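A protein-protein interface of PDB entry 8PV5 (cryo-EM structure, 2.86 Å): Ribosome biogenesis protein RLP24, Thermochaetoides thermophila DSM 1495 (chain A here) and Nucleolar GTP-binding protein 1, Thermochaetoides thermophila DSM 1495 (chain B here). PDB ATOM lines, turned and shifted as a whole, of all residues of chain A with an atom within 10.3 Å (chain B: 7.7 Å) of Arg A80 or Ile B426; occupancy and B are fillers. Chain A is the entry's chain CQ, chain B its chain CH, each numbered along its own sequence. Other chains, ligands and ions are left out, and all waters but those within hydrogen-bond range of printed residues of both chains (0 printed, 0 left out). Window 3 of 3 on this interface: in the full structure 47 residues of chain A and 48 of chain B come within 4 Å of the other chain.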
ATOM      1  N   VAL A  77     -17.317 -13.014  -1.714  1.00  0.00           N
ATOM      2  CA  VAL A  77     -16.186 -12.184  -1.307  1.00  0.00           C
ATOM      3  C   VAL A  77     -16.735 -10.877  -0.748  1.00  0.00           C
ATOM      4  O   VAL A  77     -17.265 -10.056  -1.511  1.00  0.00           O
ATOM      5  CB  VAL A  77     -15.224 -11.929  -2.477  1.00  0.00           C
ATOM      6  CG1 VAL A  77     -14.058 -11.067  -2.020  1.00  0.00           C
ATOM      7  CG2 VAL A  77     -14.728 -13.240  -3.048  1.00  0.00           C
ATOM      8  N   PRO A  78     -16.648 -10.647   0.561  1.00  0.00           N
ATOM      9  CA  PRO A  78     -17.212  -9.421   1.135  1.00  0.00           C
ATOM     10  C   PRO A  78     -16.419  -8.181   0.747  1.00  0.00           C
ATOM     11  O   PRO A  78     -15.221  -8.240   0.462  1.00  0.00           O
ATOM     12  CB  PRO A  78     -17.144  -9.677   2.644  1.00  0.00           C
ATOM     13  CG  PRO A  78     -16.041 -10.659   2.800  1.00  0.00           C
ATOM     14  CD  PRO A  78     -16.125 -11.549   1.601  1.00  0.00           C
ATOM     15  N   VAL A  79     -17.115  -7.047   0.739  1.00  0.00           N
ATOM     16  CA  VAL A  79     -16.553  -5.750   0.386  1.00  0.00           C
ATOM     17  C   VAL A  79     -16.658  -4.841   1.604  1.00  0.00           C
ATOM     18  O   VAL A  79     -17.659  -4.880   2.332  1.00  0.00           O
ATOM     19  CB  VAL A  79     -17.279  -5.148  -0.836  1.00  0.00           C
ATOM     20  CG1 VAL A  79     -16.689  -3.805  -1.234  1.00  0.00           C
ATOM     21  CG2 VAL A  79     -17.226  -6.113  -2.010  1.00  0.00           C
ATOM     22  N   ARG A  80     -15.610  -4.052   1.847  1.00  0.00           N
ATOM     23  CA  ARG A  80     -15.593  -3.126   2.973  1.00  0.00           C
ATOM     24  C   ARG A  80     -16.665  -2.054   2.798  1.00  0.00           C
ATOM     25  O   ARG A  80     -16.983  -1.648   1.677  1.00  0.00           O
ATOM     26  CB  ARG A  80     -14.203  -2.499   3.095  1.00  0.00           C
ATOM     27  CG  ARG A  80     -13.937  -1.766   4.393  1.00  0.00           C
ATOM     28  CD  ARG A  80     -12.467  -1.416   4.520  1.00  0.00           C
ATOM     29  NE  ARG A  80     -11.617  -2.590   4.356  1.00  0.00           N
ATOM     30  CZ  ARG A  80     -11.265  -3.400   5.343  1.00  0.00           C
ATOM     31  NH1 ARG A  80     -11.657  -3.187   6.587  1.00  0.00           N
ATOM     32  NH2 ARG A  80     -10.502  -4.456   5.074  1.00  0.00           N
ATOM     33  N   TYR A  81     -17.222  -1.593   3.918  1.00  0.00           N
ATOM     34  CA  TYR A  81     -18.471  -0.838   3.889  1.00  0.00           C
ATOM     35  C   TYR A  81     -18.238   0.617   3.483  1.00  0.00           C
ATOM     36  O   TYR A  81     -17.237   1.227   3.869  1.00  0.00           O
ATOM     37  CB  TYR A  81     -19.150  -0.924   5.255  1.00  0.00           C
ATOM     38  CG  TYR A  81     -20.258   0.075   5.479  1.00  0.00           C
ATOM     39  CD1 TYR A  81     -21.445  -0.001   4.764  1.00  0.00           C
ATOM     40  CD2 TYR A  81     -20.121   1.088   6.416  1.00  0.00           C
ATOM     41  CE1 TYR A  81     -22.461   0.914   4.971  1.00  0.00           C
ATOM     42  CE2 TYR A  81     -21.132   2.004   6.631  1.00  0.00           C
ATOM     43  CZ  TYR A  81     -22.297   1.911   5.907  1.00  0.00           C
ATOM     44  OH  TYR A  81     -23.305   2.823   6.120  1.00  0.00           O
ATOM     45  N   ASN A  82     -19.188   1.179   2.723  1.00  0.00           N
ATOM     46  CA  ASN A  82     -19.070   2.496   2.094  1.00  0.00           C
ATOM     47  C   ASN A  82     -20.476   3.043   1.876  1.00  0.00           C
ATOM     48  O   ASN A  82     -21.237   2.453   1.101  1.00  0.00           O
ATOM     49  CB  ASN A  82     -18.365   2.407   0.731  1.00  0.00           C
ATOM     50  CG  ASN A  82     -16.885   2.069   0.824  1.00  0.00           C
ATOM     51  OD1 ASN A  82     -16.163   2.576   1.670  1.00  0.00           O
ATOM     52  ND2 ASN A  82     -16.431   1.197  -0.070  1.00  0.00           N
ATOM     53  N   ARG A  83     -20.822   4.174   2.514  1.00  0.00           N
ATOM     54  CA  ARG A  83     -22.163   4.722   2.295  1.00  0.00           C
ATOM     55  C   ARG A  83     -22.387   5.098   0.837  1.00  0.00           C
ATOM     56  O   ARG A  83     -23.500   4.954   0.326  1.00  0.00           O
ATOM     57  CB  ARG A  83     -22.480   5.952   3.154  1.00  0.00           C
ATOM     58  CG  ARG A  83     -22.653   5.785   4.651  1.00  0.00           C
ATOM     59  CD  ARG A  83     -23.358   7.061   5.155  1.00  0.00           C
ATOM     60  NE  ARG A  83     -22.624   8.312   4.997  1.00  0.00           N
ATOM     61  CZ  ARG A  83     -21.823   8.847   5.906  1.00  0.00           C
ATOM     62  NH1 ARG A  83     -21.777   8.386   7.144  1.00  0.00           N
ATOM     63  NH2 ARG A  83     -21.096   9.914   5.583  1.00  0.00           N
ATOM     64  N   GLU A  84     -21.346   5.578   0.154  1.00  0.00           N
ATOM     65  CA  GLU A  84     -21.483   5.906  -1.262  1.00  0.00           C
ATOM     66  C   GLU A  84     -21.793   4.664  -2.091  1.00  0.00           C
ATOM     67  O   GLU A  84     -22.641   4.705  -2.994  1.00  0.00           O
ATOM     68  CB  GLU A  84     -20.211   6.590  -1.763  1.00  0.00           C
ATOM     69  CG  GLU A  84     -19.911   7.911  -1.073  1.00  0.00           C
ATOM     70  CD  GLU A  84     -20.918   8.995  -1.405  1.00  0.00           C
ATOM     71  OE1 GLU A  84     -21.470   8.981  -2.528  1.00  0.00           O
ATOM     72  OE2 GLU A  84     -21.159   9.861  -0.539  1.00  0.00           O
ATOM     73  N   LEU A  85     -21.142   3.540  -1.771  1.00  0.00           N
ATOM     74  CA  LEU A  85     -21.352   2.314  -2.532  1.00  0.00           C
ATOM     75  C   LEU A  85     -22.753   1.753  -2.307  1.00  0.00           C
ATOM     76  O   LEU A  85     -23.433   1.383  -3.267  1.00  0.00           O
ATOM     77  CB  LEU A  85     -20.286   1.281  -2.170  1.00  0.00           C
ATOM     78  CG  LEU A  85     -20.451  -0.139  -2.710  1.00  0.00           C
ATOM     79  CD1 LEU A  85     -20.475  -0.134  -4.226  1.00  0.00           C
ATOM     80  CD2 LEU A  85     -19.340  -1.035  -2.199  1.00  0.00           C
ATOM     81  N   TRP A  86     -23.215   1.706  -1.052  1.00  0.00           N
ATOM     82  CA  TRP A  86     -24.606   1.309  -0.801  1.00  0.00           C
ATOM     83  C   TRP A  86     -25.645   2.285  -1.359  1.00  0.00           C
ATOM     84  O   TRP A  86     -26.700   1.840  -1.824  1.00  0.00           O
ATOM     85  CB  TRP A  86     -24.816   1.016   0.688  1.00  0.00           C
ATOM     86  CG  TRP A  86     -24.421  -0.397   1.101  1.00  0.00           C
ATOM     87  CD1 TRP A  86     -25.287  -1.446   1.219  1.00  0.00           C
ATOM     88  CD2 TRP A  86     -23.108  -0.974   1.176  1.00  0.00           C
ATOM     89  NE1 TRP A  86     -24.613  -2.597   1.521  1.00  0.00           N
ATOM     90  CE2 TRP A  86     -23.270  -2.340   1.485  1.00  0.00           C
ATOM     91  CE3 TRP A  86     -21.818  -0.465   1.076  1.00  0.00           C
ATOM     92  CZ2 TRP A  86     -22.191  -3.193   1.681  1.00  0.00           C
ATOM     93  CZ3 TRP A  86     -20.752  -1.310   1.274  1.00  0.00           C
ATOM     94  CH2 TRP A  86     -20.941  -2.658   1.578  1.00  0.00           C
ATOM     95  N   THR A  89     -25.683   1.696  -4.986  1.00  0.00           N
ATOM     96  CA  THR A  89     -26.245   0.361  -5.144  1.00  0.00           C
ATOM     97  C   THR A  89     -27.765   0.389  -5.085  1.00  0.00           C
ATOM     98  O   THR A  89     -28.425  -0.261  -5.896  1.00  0.00           O
ATOM     99  CB  THR A  89     -25.677  -0.567  -4.071  1.00  0.00           C
ATOM    100  OG1 THR A  89     -24.257  -0.659  -4.230  1.00  0.00           O
ATOM    101  CG2 THR A  89     -26.280  -1.959  -4.183  1.00  0.00           C
ATOM    102  N   ARG B 422     -18.623  -2.852  16.650  1.00  0.00           N
ATOM    103  CA  ARG B 422     -18.202  -1.961  15.580  1.00  0.00           C
ATOM    104  C   ARG B 422     -17.092  -1.013  16.006  1.00  0.00           C
ATOM    105  O   ARG B 422     -16.720  -0.129  15.229  1.00  0.00           O
ATOM    106  CB  ARG B 422     -19.399  -1.158  15.066  1.00  0.00           C
ATOM    107  CG  ARG B 422     -20.674  -1.971  14.968  1.00  0.00           C
ATOM    108  CD  ARG B 422     -21.881  -1.087  14.742  1.00  0.00           C
ATOM    109  NE  ARG B 422     -21.965  -0.631  13.360  1.00  0.00           N
ATOM    110  CZ  ARG B 422     -22.885  -1.037  12.498  1.00  0.00           C
ATOM    111  NH1 ARG B 422     -23.822  -1.903  12.843  1.00  0.00           N
ATOM    112  NH2 ARG B 422     -22.864  -0.560  11.256  1.00  0.00           N
ATOM    113  N   LYS B 423     -16.573  -1.165  17.227  1.00  0.00           N
ATOM    114  CA  LYS B 423     -15.494  -0.301  17.696  1.00  0.00           C
ATOM    115  C   LYS B 423     -14.201  -0.557  16.935  1.00  0.00           C
ATOM    116  O   LYS B 423     -13.493   0.386  16.562  1.00  0.00           O
ATOM    117  CB  LYS B 423     -15.279  -0.509  19.195  1.00  0.00           C
ATOM    118  CG  LYS B 423     -14.202   0.374  19.799  1.00  0.00           C
ATOM    119  CD  LYS B 423     -14.137   0.206  21.306  1.00  0.00           C
ATOM    120  CE  LYS B 423     -13.519  -1.130  21.683  1.00  0.00           C
ATOM    121  NZ  LYS B 423     -13.339  -1.262  23.155  1.00  0.00           N
ATOM    122  N   ASP B 424     -13.874  -1.826  16.691  1.00  0.00           N
ATOM    123  CA  ASP B 424     -12.631  -2.201  16.032  1.00  0.00           C
ATOM    124  C   ASP B 424     -12.788  -2.345  14.523  1.00  0.00           C
ATOM    125  O   ASP B 424     -12.025  -3.089  13.896  1.00  0.00           O
ATOM    126  CB  ASP B 424     -12.087  -3.496  16.634  1.00  0.00           C
ATOM    127  CG  ASP B 424     -11.537  -3.301  18.031  1.00  0.00           C
ATOM    128  OD1 ASP B 424     -11.441  -2.139  18.475  1.00  0.00           O
ATOM    129  OD2 ASP B 424     -11.200  -4.311  18.685  1.00  0.00           O
ATOM    130  N   TRP B 425     -13.759  -1.657  13.931  1.00  0.00           N
ATOM    131  CA  TRP B 425     -13.921  -1.685  12.485  1.00  0.00           C
ATOM    132  C   TRP B 425     -12.840  -0.853  11.810  1.00  0.00           C
ATOM    133  O   TRP B 425     -12.535   0.264  12.234  1.00  0.00           O
ATOM    134  CB  TRP B 425     -15.299  -1.158  12.093  1.00  0.00           C
ATOM    135  CG  TRP B 425     -16.354  -2.211  12.034  1.00  0.00           C
ATOM    136  CD1 TRP B 425     -16.265  -3.489  12.499  1.00  0.00           C
ATOM    137  CD2 TRP B 425     -17.666  -2.077  11.477  1.00  0.00           C
ATOM    138  NE1 TRP B 425     -17.439  -4.161  12.266  1.00  0.00           N
ATOM    139  CE2 TRP B 425     -18.316  -3.314  11.639  1.00  0.00           C
ATOM    140  CE3 TRP B 425     -18.353  -1.029  10.857  1.00  0.00           C
ATOM    141  CZ2 TRP B 425     -19.620  -3.533  11.204  1.00  0.00           C
ATOM    142  CZ3 TRP B 425     -19.648  -1.249  10.428  1.00  0.00           C
ATOM    143  CH2 TRP B 425     -20.267  -2.491  10.602  1.00  0.00           C
ATOM    144  N   ILE B 426     -12.258  -1.406  10.751  1.00  0.00           N
ATOM    145  CA  ILE B 426     -11.257  -0.720   9.945  1.00  0.00           C
ATOM    146  C   ILE B 426     -11.947  -0.262   8.670  1.00  0.00           C
ATOM    147  O   ILE B 426     -12.218  -1.072   7.776  1.00  0.00           O
ATOM    148  CB  ILE B 426     -10.056  -1.621   9.632  1.00  0.00           C
ATOM    149  CG1 ILE B 426      -9.425  -2.145  10.921  1.00  0.00           C
ATOM    150  CG2 ILE B 426      -9.028  -0.867   8.805  1.00  0.00           C
ATOM    151  CD1 ILE B 426      -8.456  -3.282  10.703  1.00  0.00           C
ATOM    152  N   LEU B 427     -12.236   1.032   8.582  1.00  0.00           N
ATOM    153  CA  LEU B 427     -12.921   1.601   7.433  1.00  0.00           C
ATOM    154  C   LEU B 427     -12.101   2.747   6.856  1.00  0.00           C
ATOM    155  O   LEU B 427     -11.212   3.295   7.513  1.00  0.00           O
ATOM    156  CB  LEU B 427     -14.326   2.094   7.805  1.00  0.00           C
ATOM    157  CG  LEU B 427     -15.302   1.032   8.319  1.00  0.00           C
ATOM    158  CD1 LEU B 427     -16.662   1.640   8.583  1.00  0.00           C
ATOM    159  CD2 LEU B 427     -15.421  -0.126   7.352  1.00  0.00           C
ATOM    160  N   GLU B 428     -12.404   3.089   5.601  1.00  0.00           N
ATOM    161  CA  GLU B 428     -11.712   4.194   4.942  1.00  0.00           C
ATOM    162  C   GLU B 428     -12.052   5.527   5.595  1.00  0.00           C
ATOM    163  O   GLU B 428     -11.179   6.385   5.765  1.00  0.00           O
ATOM    164  CB  GLU B 428     -12.060   4.224   3.454  1.00  0.00           C
ATOM    165  CG  GLU B 428     -11.518   3.052   2.648  1.00  0.00           C
ATOM    166  CD  GLU B 428     -12.440   1.848   2.659  1.00  0.00           C
ATOM    167  OE1 GLU B 428     -13.524   1.928   3.274  1.00  0.00           O
ATOM    168  OE2 GLU B 428     -12.080   0.819   2.048  1.00  0.00           O
ATOM    169  N   ASN B 429     -13.315   5.717   5.967  1.00  0.00           N
ATOM    170  CA  ASN B 429     -13.780   6.949   6.591  1.00  0.00           C
ATOM    171  C   ASN B 429     -14.159   6.624   8.030  1.00  0.00           C
ATOM    172  O   ASN B 429     -14.787   5.580   8.278  1.00  0.00           O
ATOM    173  CB  ASN B 429     -14.957   7.531   5.789  1.00  0.00           C
ATOM    174  CG  ASN B 429     -15.658   8.712   6.467  1.00  0.00           C
ATOM    175  OD1 ASN B 429     -16.239   8.598   7.546  1.00  0.00           O
ATOM    176  ND2 ASN B 429     -15.610   9.862   5.807  1.00  0.00           N
ATOM    177  N   TRP B 432     -18.162   6.198   9.496  1.00  0.00           N
ATOM    178  CA  TRP B 432     -19.028   5.165   8.943  1.00  0.00           C
ATOM    179  C   TRP B 432     -19.191   3.972   9.871  1.00  0.00           C
ATOM    180  O   TRP B 432     -20.066   3.137   9.632  1.00  0.00           O
ATOM    181  CB  TRP B 432     -18.500   4.675   7.591  1.00  0.00           C
ATOM    182  CG  TRP B 432     -18.519   5.700   6.521  1.00  0.00           C
ATOM    183  CD1 TRP B 432     -19.227   6.851   6.518  1.00  0.00           C
ATOM    184  CD2 TRP B 432     -17.820   5.654   5.273  1.00  0.00           C
ATOM    185  NE1 TRP B 432     -19.008   7.545   5.355  1.00  0.00           N
ATOM    186  CE2 TRP B 432     -18.145   6.830   4.572  1.00  0.00           C
ATOM    187  CE3 TRP B 432     -16.940   4.743   4.689  1.00  0.00           C
ATOM    188  CZ2 TRP B 432     -17.623   7.117   3.315  1.00  0.00           C
ATOM    189  CZ3 TRP B 432     -16.421   5.033   3.446  1.00  0.00           C
ATOM    190  CH2 TRP B 432     -16.768   6.205   2.769  1.00  0.00           C
ATOM    191  N   LYS B 433     -18.380   3.872  10.922  1.00  0.00           N
ATOM    192  CA  LYS B 433     -18.378   2.659  11.726  1.00  0.00           C
ATOM    193  C   LYS B 433     -19.602   2.545  12.631  1.00  0.00           C
ATOM    194  O   LYS B 433     -19.866   1.459  13.154  1.00  0.00           O
ATOM    195  CB  LYS B 433     -17.091   2.592  12.551  1.00  0.00           C
ATOM    196  CG  LYS B 433     -16.939   3.711  13.583  1.00  0.00           C
ATOM    197  CD  LYS B 433     -15.502   3.838  14.107  1.00  0.00           C
ATOM    198  CE  LYS B 433     -14.890   2.479  14.419  1.00  0.00           C
ATOM    199  NZ  LYS B 433     -13.450   2.573  14.783  1.00  0.00           N
ATOM    200  N   ILE B 450     -24.551  -5.823  -4.208  1.00  0.00           N
ATOM    201  CA  ILE B 450     -23.310  -5.124  -3.889  1.00  0.00           C
ATOM    202  C   ILE B 450     -22.198  -5.631  -4.797  1.00  0.00           C
ATOM    203  O   ILE B 450     -21.937  -6.838  -4.874  1.00  0.00           O
ATOM    204  CB  ILE B 450     -22.955  -5.289  -2.406  1.00  0.00           C
ATOM    205  CG1 ILE B 450     -23.772  -4.315  -1.565  1.00  0.00           C
ATOM    206  CG2 ILE B 450     -21.470  -5.054  -2.160  1.00  0.00           C
ATOM    207  CD1 ILE B 450     -23.494  -2.876  -1.904  1.00  0.00           C
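NH1 of Arg A80 sits at hydrogen-bond distance from O of Ile B426, at 2.5 Å. OD1 of Asn A82 sits close to OE1 of Glu B428 (3.2 Å). The guanidinium group (NH2) of Arg A83 sits close to the indole nitrogen (NE1) of Trp B432.
Among the printed residues, merely in contact across the chains: Asn A82 with Trp B432, Thr A89 with Ile B450, Arg A80 with Glu B428, Tyr A81 with Trp B432, Trp A86 with Ile B450, Arg A80 with Leu B427 and Tyr A81 with Glu B428.
The side-chain amide nitrogen of Asn A82 is in hydrogen-bond range of the backbone carbonyl oxygen of Arg A80 (3.4 Å). The backbone carbonyl oxygen (O) of Leu A85 sits at hydrogen-bond distance from the side-chain hydroxyl (OG1) of Thr A89 (2.4 Å).
Hydrophobic or aromatic side chains of chain B within 4 Å of the printed part of chain A: Ile B426, Leu B427, Trp B432 and Ile B450. Of the 11 printed residues of chain A, 6 touch a printed residue of chain B. Hydrophobic or aromatic side chains of chain A that line the printed part of chain B: Tyr A81 and Trp A86. Among the printed residues, no Asp or Glu carboxylate lies within 4 Å of a Lys or Arg side-chain nitrogen of the other chain.
Of chain B, only Ile B426 (2.5 Å), Leu B427 (3.7 Å) and Glu B428 (3.4 Å) come within 4 Å of Arg A80. Of the printed residues of chain B, Asn A82 touches Glu B428 and Trp B432. Leu A85 touches none of the printed residues of chain B. Of the printed residues of chain B, Trp A86 touches Ile B450 (3.4 Å). Of the printed residues of chain B, Thr A89 touches Ile B450 (3.3 Å). Ile B426 touches just one residue of chain A: Arg A80. Leu B427 touches just one residue of chain A: Arg A80 (3.7 Å). The nearest residue of chain B that does not touch Arg A80 is Trp B425 (5.8 Å). The nearest residue of chain A that does not touch Ile B426 is Tyr A81 (6.3 Å).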
